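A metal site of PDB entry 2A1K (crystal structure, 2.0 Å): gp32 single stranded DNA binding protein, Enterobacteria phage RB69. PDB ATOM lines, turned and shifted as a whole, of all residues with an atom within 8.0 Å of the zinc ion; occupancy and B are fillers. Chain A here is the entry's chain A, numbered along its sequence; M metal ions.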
ATOM      1  N   VAL A  42      -6.592  -0.120  -6.355  1.00  0.00           N
ATOM      2  CA  VAL A  42      -7.237  -1.311  -6.913  1.00  0.00           C
ATOM      3  C   VAL A  42      -8.476  -0.838  -7.659  1.00  0.00           C
ATOM      4  O   VAL A  42      -9.065   0.181  -7.328  1.00  0.00           O
ATOM      5  CB  VAL A  42      -7.685  -2.290  -5.786  1.00  0.00           C
ATOM      6  CG1 VAL A  42      -8.153  -3.615  -6.408  1.00  0.00           C
ATOM      7  CG2 VAL A  42      -6.542  -2.532  -4.821  1.00  0.00           C
ATOM      8  N   ASN A  43      -8.862  -1.559  -8.713  1.00  0.00           N
ATOM      9  CA  ASN A  43     -10.056  -1.190  -9.465  1.00  0.00           C
ATOM     10  C   ASN A  43     -10.514  -2.287 -10.403  1.00  0.00           C
ATOM     11  O   ASN A  43      -9.876  -3.336 -10.504  1.00  0.00           O
ATOM     12  CB  ASN A  43      -9.824   0.121 -10.223  1.00  0.00           C
ATOM     13  CG  ASN A  43      -8.523   0.140 -10.982  1.00  0.00           C
ATOM     14  OD1 ASN A  43      -7.778   1.123 -10.918  1.00  0.00           O
ATOM     15  ND2 ASN A  43      -8.248  -0.932 -11.707  1.00  0.00           N
ATOM     16  N   HIS A  44     -11.648  -2.037 -11.061  1.00  0.00           N
ATOM     17  CA  HIS A  44     -12.230  -2.975 -12.010  1.00  0.00           C
ATOM     18  C   HIS A  44     -12.385  -2.311 -13.372  1.00  0.00           C
ATOM     19  O   HIS A  44     -12.599  -1.110 -13.459  1.00  0.00           O
ATOM     20  CB  HIS A  44     -13.604  -3.441 -11.521  1.00  0.00           C
ATOM     21  CG  HIS A  44     -13.560  -4.182 -10.231  1.00  0.00           C
ATOM     22  ND1 HIS A  44     -13.184  -5.507 -10.141  1.00  0.00           N
ATOM     23  CD2 HIS A  44     -13.821  -3.785  -8.958  1.00  0.00           C
ATOM     24  CE1 HIS A  44     -13.216  -5.886  -8.875  1.00  0.00           C
ATOM     25  NE2 HIS A  44     -13.591  -4.860  -8.138  1.00  0.00           N
ATOM     26  N   TYR A  53     -17.549  -0.713 -17.447  1.00  0.00           N
ATOM     27  CA  TYR A  53     -17.592  -0.490 -16.015  1.00  0.00           C
ATOM     28  C   TYR A  53     -16.117  -0.294 -15.674  1.00  0.00           C
ATOM     29  O   TYR A  53     -15.323  -1.247 -15.719  1.00  0.00           O
ATOM     30  CB  TYR A  53     -18.147  -1.694 -15.251  1.00  0.00           C
ATOM     31  CG  TYR A  53     -18.210  -1.454 -13.759  1.00  0.00           C
ATOM     32  CD1 TYR A  53     -17.078  -1.627 -12.951  1.00  0.00           C
ATOM     33  CD2 TYR A  53     -19.373  -1.019 -13.152  1.00  0.00           C
ATOM     34  CE1 TYR A  53     -17.118  -1.366 -11.578  1.00  0.00           C
ATOM     35  CE2 TYR A  53     -19.433  -0.752 -11.804  1.00  0.00           C
ATOM     36  CZ  TYR A  53     -18.304  -0.925 -11.011  1.00  0.00           C
ATOM     37  OH  TYR A  53     -18.373  -0.622  -9.670  1.00  0.00           O
ATOM     38  N   GLU A  55     -14.214   1.521 -12.649  1.00  0.00           N
ATOM     39  CA  GLU A  55     -14.300   2.213 -11.366  1.00  0.00           C
ATOM     40  C   GLU A  55     -13.252   1.757 -10.363  1.00  0.00           C
ATOM     41  O   GLU A  55     -12.709   0.648 -10.467  1.00  0.00           O
ATOM     42  CB  GLU A  55     -15.673   1.963 -10.739  1.00  0.00           C
ATOM     43  CG  GLU A  55     -16.856   2.415 -11.559  1.00  0.00           C
ATOM     44  CD  GLU A  55     -17.066   3.914 -11.496  1.00  0.00           C
ATOM     45  OE1 GLU A  55     -16.623   4.549 -10.515  1.00  0.00           O
ATOM     46  OE2 GLU A  55     -17.709   4.462 -12.423  1.00  0.00           O
ATOM     47  N   THR A  56     -12.980   2.598  -9.378  1.00  0.00           N
ATOM     48  CA  THR A  56     -12.035   2.236  -8.337  1.00  0.00           C
ATOM     49  C   THR A  56     -12.774   1.239  -7.453  1.00  0.00           C
ATOM     50  O   THR A  56     -14.015   1.237  -7.410  1.00  0.00           O
ATOM     51  CB  THR A  56     -11.637   3.452  -7.492  1.00  0.00           C
ATOM     52  OG1 THR A  56     -12.827   4.126  -7.059  1.00  0.00           O
ATOM     53  CG2 THR A  56     -10.765   4.419  -8.314  1.00  0.00           C
ATOM     54  N   CYS A  57     -12.011   0.410  -6.763  1.00  0.00           N
ATOM     55  CA  CYS A  57     -12.574  -0.606  -5.866  1.00  0.00           C
ATOM     56  C   CYS A  57     -12.279  -0.252  -4.412  1.00  0.00           C
ATOM     57  O   CYS A  57     -11.119  -0.075  -4.021  1.00  0.00           O
ATOM     58  CB  CYS A  57     -12.002  -1.989  -6.184  1.00  0.00           C
ATOM     59  SG  CYS A  57     -12.513  -3.292  -5.052  1.00  0.00           S
ATOM     60  N   SER A  58     -13.329  -0.164  -3.608  1.00  0.00           N
ATOM     61  CA  SER A  58     -13.194   0.172  -2.197  1.00  0.00           C
ATOM     62  C   SER A  58     -12.300  -0.795  -1.405  1.00  0.00           C
ATOM     63  O   SER A  58     -11.984  -0.538  -0.239  1.00  0.00           O
ATOM     64  CB  SER A  58     -14.586   0.280  -1.548  1.00  0.00           C
ATOM     65  OG  SER A  58     -15.381  -0.848  -1.864  1.00  0.00           O
ATOM     66  N   SER A  59     -11.869  -1.903  -2.028  1.00  0.00           N
ATOM     67  CA  SER A  59     -10.991  -2.855  -1.334  1.00  0.00           C
ATOM     68  C   SER A  59      -9.607  -2.241  -1.232  1.00  0.00           C
ATOM     69  O   SER A  59      -8.724  -2.770  -0.564  1.00  0.00           O
ATOM     70  CB  SER A  59     -10.927  -4.200  -2.072  1.00  0.00           C
ATOM     71  OG  SER A  59     -10.040  -4.161  -3.180  1.00  0.00           O
ATOM     72  N   THR A  60      -9.414  -1.108  -1.914  1.00  0.00           N
ATOM     73  CA  THR A  60      -8.126  -0.421  -1.861  1.00  0.00           C
ATOM     74  C   THR A  60      -7.835  -0.077  -0.399  1.00  0.00           C
ATOM     75  O   THR A  60      -6.685  -0.101   0.028  1.00  0.00           O
ATOM     76  CB  THR A  60      -8.162   0.871  -2.679  1.00  0.00           C
ATOM     77  OG1 THR A  60      -8.497   0.561  -4.034  1.00  0.00           O
ATOM     78  CG2 THR A  60      -6.813   1.551  -2.630  1.00  0.00           C
ATOM     79  N   ASP A  63     -12.219  -2.258   2.090  1.00  0.00           N
ATOM     80  CA  ASP A  63     -13.671  -2.324   2.115  1.00  0.00           C
ATOM     81  C   ASP A  63     -14.261  -3.029   0.896  1.00  0.00           C
ATOM     82  O   ASP A  63     -14.562  -2.396  -0.116  1.00  0.00           O
ATOM     83  CB  ASP A  63     -14.213  -0.895   2.239  1.00  0.00           C
ATOM     84  CG  ASP A  63     -15.731  -0.825   2.251  1.00  0.00           C
ATOM     85  OD1 ASP A  63     -16.400  -1.874   2.334  1.00  0.00           O
ATOM     86  OD2 ASP A  63     -16.258   0.303   2.194  1.00  0.00           O
ATOM     87  N   TYR A  64     -14.444  -4.341   1.006  1.00  0.00           N
ATOM     88  CA  TYR A  64     -15.011  -5.141  -0.071  1.00  0.00           C
ATOM     89  C   TYR A  64     -16.532  -5.018  -0.161  1.00  0.00           C
ATOM     90  O   TYR A  64     -17.115  -5.291  -1.199  1.00  0.00           O
ATOM     91  CB  TYR A  64     -14.673  -6.620   0.101  1.00  0.00           C
ATOM     92  CG  TYR A  64     -13.235  -6.971  -0.162  1.00  0.00           C
ATOM     93  CD1 TYR A  64     -12.282  -6.933   0.859  1.00  0.00           C
ATOM     94  CD2 TYR A  64     -12.823  -7.328  -1.441  1.00  0.00           C
ATOM     95  CE1 TYR A  64     -10.941  -7.250   0.605  1.00  0.00           C
ATOM     96  CE2 TYR A  64     -11.492  -7.632  -1.708  1.00  0.00           C
ATOM     97  CZ  TYR A  64     -10.561  -7.598  -0.690  1.00  0.00           C
ATOM     98  OH  TYR A  64      -9.252  -7.865  -0.968  1.00  0.00           O
ATOM     99  N   ASP A  65     -17.172  -4.643   0.943  1.00  0.00           N
ATOM    100  CA  ASP A  65     -18.629  -4.503   0.992  1.00  0.00           C
ATOM    101  C   ASP A  65     -19.175  -3.376   0.119  1.00  0.00           C
ATOM    102  O   ASP A  65     -20.275  -3.479  -0.414  1.00  0.00           O
ATOM    103  CB  ASP A  65     -19.105  -4.288   2.430  1.00  0.00           C
ATOM    104  CG  ASP A  65     -18.979  -5.543   3.281  1.00  0.00           C
ATOM    105  OD1 ASP A  65     -18.544  -5.422   4.436  1.00  0.00           O
ATOM    106  OD2 ASP A  65     -19.329  -6.630   2.812  1.00  0.00           O
ATOM    107  N   SER A  66     -18.400  -2.301   0.002  1.00  0.00           N
ATOM    108  CA  SER A  66     -18.845  -1.152  -0.768  1.00  0.00           C
ATOM    109  C   SER A  66     -18.595  -1.250  -2.262  1.00  0.00           C
ATOM    110  O   SER A  66     -18.797  -0.279  -2.998  1.00  0.00           O
ATOM    111  CB  SER A  66     -18.189   0.119  -0.222  1.00  0.00           C
ATOM    112  OG  SER A  66     -18.644   0.338   1.097  1.00  0.00           O
ATOM    113  N   CYS A  67     -18.163  -2.426  -2.718  1.00  0.00           N
ATOM    114  CA  CYS A  67     -17.916  -2.637  -4.129  1.00  0.00           C
ATOM    115  C   CYS A  67     -18.880  -3.697  -4.647  1.00  0.00           C
ATOM    116  O   CYS A  67     -18.859  -4.842  -4.204  1.00  0.00           O
ATOM    117  CB  CYS A  67     -16.486  -3.108  -4.359  1.00  0.00           C
ATOM    118  SG  CYS A  67     -16.177  -3.440  -6.094  1.00  0.00           S
ATOM    119  N   PRO A  68     -19.747  -3.323  -5.608  1.00  0.00           N
ATOM    120  CA  PRO A  68     -20.725  -4.250  -6.177  1.00  0.00           C
ATOM    121  C   PRO A  68     -20.120  -5.398  -6.974  1.00  0.00           C
ATOM    122  O   PRO A  68     -20.649  -6.508  -7.001  1.00  0.00           O
ATOM    123  CB  PRO A  68     -21.593  -3.337  -7.052  1.00  0.00           C
ATOM    124  CG  PRO A  68     -21.369  -1.962  -6.474  1.00  0.00           C
ATOM    125  CD  PRO A  68     -19.900  -1.989  -6.198  1.00  0.00           C
ATOM    126  N   VAL A  69     -19.002  -5.121  -7.642  1.00  0.00           N
ATOM    127  CA  VAL A  69     -18.320  -6.131  -8.428  1.00  0.00           C
ATOM    128  C   VAL A  69     -17.800  -7.242  -7.521  1.00  0.00           C
ATOM    129  O   VAL A  69     -18.118  -8.412  -7.707  1.00  0.00           O
ATOM    130  CB  VAL A  69     -17.146  -5.504  -9.193  1.00  0.00           C
ATOM    131  CG1 VAL A  69     -16.601  -6.492 -10.199  1.00  0.00           C
ATOM    132  CG2 VAL A  69     -17.613  -4.220  -9.869  1.00  0.00           C
ATOM    133  N   CYS A  70     -16.998  -6.857  -6.533  1.00  0.00           N
ATOM    134  CA  CYS A  70     -16.476  -7.825  -5.573  1.00  0.00           C
ATOM    135  C   CYS A  70     -17.640  -8.606  -4.956  1.00  0.00           C
ATOM    136  O   CYS A  70     -17.534  -9.818  -4.742  1.00  0.00           O
ATOM    137  CB  CYS A  70     -15.706  -7.111  -4.473  1.00  0.00           C
ATOM    138  SG  CYS A  70     -14.023  -6.691  -4.929  1.00  0.00           S
ATOM    139  N   GLN A  71     -18.747  -7.932  -4.689  1.00  0.00           N
ATOM    140  CA  GLN A  71     -19.900  -8.599  -4.112  1.00  0.00           C
ATOM    141  C   GLN A  71     -20.425  -9.649  -5.083  1.00  0.00           C
ATOM    142  O   GLN A  71     -20.711 -10.779  -4.686  1.00  0.00           O
ATOM    143  CB  GLN A  71     -20.991  -7.592  -3.778  1.00  0.00           C
ATOM    144  CG  GLN A  71     -20.647  -6.733  -2.612  1.00  0.00           C
ATOM    145  CD  GLN A  71     -20.263  -7.552  -1.402  1.00  0.00           C
ATOM    146  OE1 GLN A  71     -21.091  -8.269  -0.839  1.00  0.00           O
ATOM    147  NE2 GLN A  71     -19.000  -7.457  -1.005  1.00  0.00           N
ATOM    148  N   TYR A  72     -20.528  -9.254  -6.347  1.00  0.00           N
ATOM    149  CA  TYR A  72     -21.018 -10.126  -7.407  1.00  0.00           C
ATOM    150  C   TYR A  72     -20.078 -11.306  -7.581  1.00  0.00           C
ATOM    151  O   TYR A  72     -20.508 -12.462  -7.581  1.00  0.00           O
ATOM    152  CB  TYR A  72     -21.096  -9.353  -8.722  1.00  0.00           C
ATOM    153  CG  TYR A  72     -21.733 -10.130  -9.852  1.00  0.00           C
ATOM    154  CD1 TYR A  72     -23.128 -10.186  -9.981  1.00  0.00           C
ATOM    155  CD2 TYR A  72     -20.956 -10.798 -10.786  1.00  0.00           C
ATOM    156  CE1 TYR A  72     -23.720 -10.889 -11.028  1.00  0.00           C
ATOM    157  CE2 TYR A  72     -21.546 -11.507 -11.840  1.00  0.00           C
ATOM    158  CZ  TYR A  72     -22.930 -11.534 -11.950  1.00  0.00           C
ATOM    159  OH  TYR A  72     -23.515 -12.226 -12.991  1.00  0.00           O
ATOM    160  N   ILE A  73     -18.791 -11.007  -7.733  1.00  0.00           N
ATOM    161  CA  ILE A  73     -17.781 -12.044  -7.916  1.00  0.00           C
ATOM    162  C   ILE A  73     -17.874 -13.074  -6.780  1.00  0.00           C
ATOM    163  O   ILE A  73     -17.923 -14.273  -7.027  1.00  0.00           O
ATOM    164  CB  ILE A  73     -16.362 -11.417  -7.950  1.00  0.00           C
ATOM    165  CG1 ILE A  73     -16.254 -10.479  -9.151  1.00  0.00           C
ATOM    166  CG2 ILE A  73     -15.285 -12.508  -7.999  1.00  0.00           C
ATOM    167  CD1 ILE A  73     -14.957  -9.729  -9.231  1.00  0.00           C
ATOM    168  N   LEU A  89     -13.731  -9.691 -14.626  1.00  0.00           N
ATOM    169  CA  LEU A  89     -14.175  -8.816 -13.534  1.00  0.00           C
ATOM    170  C   LEU A  89     -13.265  -8.630 -12.315  1.00  0.00           C
ATOM    171  O   LEU A  89     -13.484  -7.718 -11.517  1.00  0.00           O
ATOM    172  CB  LEU A  89     -15.553  -9.276 -13.052  1.00  0.00           C
ATOM    173  CG  LEU A  89     -16.811  -8.937 -13.863  1.00  0.00           C
ATOM    174  CD1 LEU A  89     -16.768  -9.531 -15.271  1.00  0.00           C
ATOM    175  CD2 LEU A  89     -18.012  -9.450 -13.095  1.00  0.00           C
ATOM    176  N   LYS A  90     -12.252  -9.472 -12.166  1.00  0.00           N
ATOM    177  CA  LYS A  90     -11.357  -9.403 -10.999  1.00  0.00           C
ATOM    178  C   LYS A  90     -10.723  -8.044 -10.738  1.00  0.00           C
ATOM    179  O   LYS A  90     -10.463  -7.268 -11.675  1.00  0.00           O
ATOM    180  CB  LYS A  90     -10.250 -10.448 -11.119  1.00  0.00           C
ATOM    181  CG  LYS A  90      -9.255 -10.166 -12.232  1.00  0.00           C
ATOM    182  CD  LYS A  90      -8.211 -11.276 -12.383  1.00  0.00           C
ATOM    183  CE  LYS A  90      -7.470 -11.155 -13.712  1.00  0.00           C
ATOM    184  NZ  LYS A  90      -6.567 -12.300 -13.980  1.00  0.00           N
ATOM    185  N   ARG A  91     -10.464  -7.752  -9.470  1.00  0.00           N
ATOM    186  CA  ARG A  91      -9.829  -6.488  -9.114  1.00  0.00           C
ATOM    187  C   ARG A  91      -8.420  -6.438  -9.706  1.00  0.00           C
ATOM    188  O   ARG A  91      -7.755  -7.459  -9.892  1.00  0.00           O
ATOM    189  CB  ARG A  91      -9.792  -6.310  -7.581  1.00  0.00           C
ATOM    190  CG  ARG A  91      -9.929  -7.589  -6.782  1.00  0.00           C
ATOM    191  CD  ARG A  91     -10.338  -7.323  -5.329  1.00  0.00           C
ATOM    192  NE  ARG A  91      -9.277  -6.636  -4.596  1.00  0.00           N
ATOM    193  CZ  ARG A  91      -8.074  -7.141  -4.360  1.00  0.00           C
ATOM    194  NH1 ARG A  91      -7.758  -8.355  -4.802  1.00  0.00           N
ATOM    195  NH2 ARG A  91      -7.170  -6.428  -3.707  1.00  0.00           N
ATOM    196  N   LYS A  92      -7.981  -5.230 -10.047  1.00  0.00           N
ATOM    197  CA  LYS A  92      -6.663  -5.012 -10.634  1.00  0.00           C
ATOM    198  C   LYS A  92      -5.900  -3.968  -9.821  1.00  0.00           C
ATOM    199  O   LYS A  92      -6.394  -2.866  -9.603  1.00  0.00           O
ATOM    200  CB  LYS A  92      -6.804  -4.552 -12.086  1.00  0.00           C
ATOM    201  CG  LYS A  92      -7.391  -5.616 -12.995  1.00  0.00           C
ATOM    202  CD  LYS A  92      -7.552  -5.135 -14.431  1.00  0.00           C
ATOM    203  CE  LYS A  92      -8.086  -6.278 -15.296  1.00  0.00           C
ATOM    204  NZ  LYS A  92      -8.206  -5.912 -16.729  1.00  0.00           N
ATOM    205  N   LEU A 211     -22.391   2.853  -7.754  1.00  0.00           N
ATOM    206  CA  LEU A 211     -21.652   1.801  -8.420  1.00  0.00           C
ATOM    207  C   LEU A 211     -22.560   0.642  -8.808  1.00  0.00           C
ATOM    208  O   LEU A 211     -22.481   0.127  -9.923  1.00  0.00           O
ATOM    209  CB  LEU A 211     -20.538   1.274  -7.513  1.00  0.00           C
ATOM    210  CG  LEU A 211     -19.444   2.288  -7.175  1.00  0.00           C
ATOM    211  CD1 LEU A 211     -18.388   1.620  -6.312  1.00  0.00           C
ATOM    212  CD2 LEU A 211     -18.824   2.814  -8.457  1.00  0.00           C
HETATM  213 ZN    ZN M   1     -14.148  -4.616  -6.018  1.00  0.00          ZN
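NE2 of His 44 binds the zinc ion (2.2 Å). The zinc ion is bound by SG of Cys 57 (2.3 Å). SG of Cys 67 binds the zinc ion (2.3 Å). SG of Cys 70 binds the zinc ion.
Four residues have an atom within 4 Å of the zinc ion: His 44, Cys 57, Cys 67 and Cys 70. Along chain A the residues within 4 Å of the zinc ion span positions 44 to 70. The nearest printed residue that does not touch the zinc ion is Val 69 (4.5 Å).
A ring nitrogen (ND1) of His 44 sits at hydrogen-bond distance from the backbone carbonyl oxygen (O) of Leu 89, at 2.6 Å. The backbone NH of His 44 lies within hydrogen-bond range of the backbone carbonyl oxygen of Glu 55 (2.9 Å). The side-chain sulfur of Cys 57 lies close to the side-chain hydroxyl of Ser 59. The backbone NH of Cys 57 lies within hydrogen-bond range of the backbone carbonyl oxygen of Val 42 (3.0 Å). O of Cys 57 lies within hydrogen-bond range of OG1 of Thr 60 (2.7 Å). The side-chain sulfur (SG) of Cys 67 sits close to the backbone NH (N) of Val 69. The backbone NH (N) of Cys 67 sits at hydrogen-bond distance from the side-chain hydroxyl (OG) of Ser 58 (3.3 Å).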
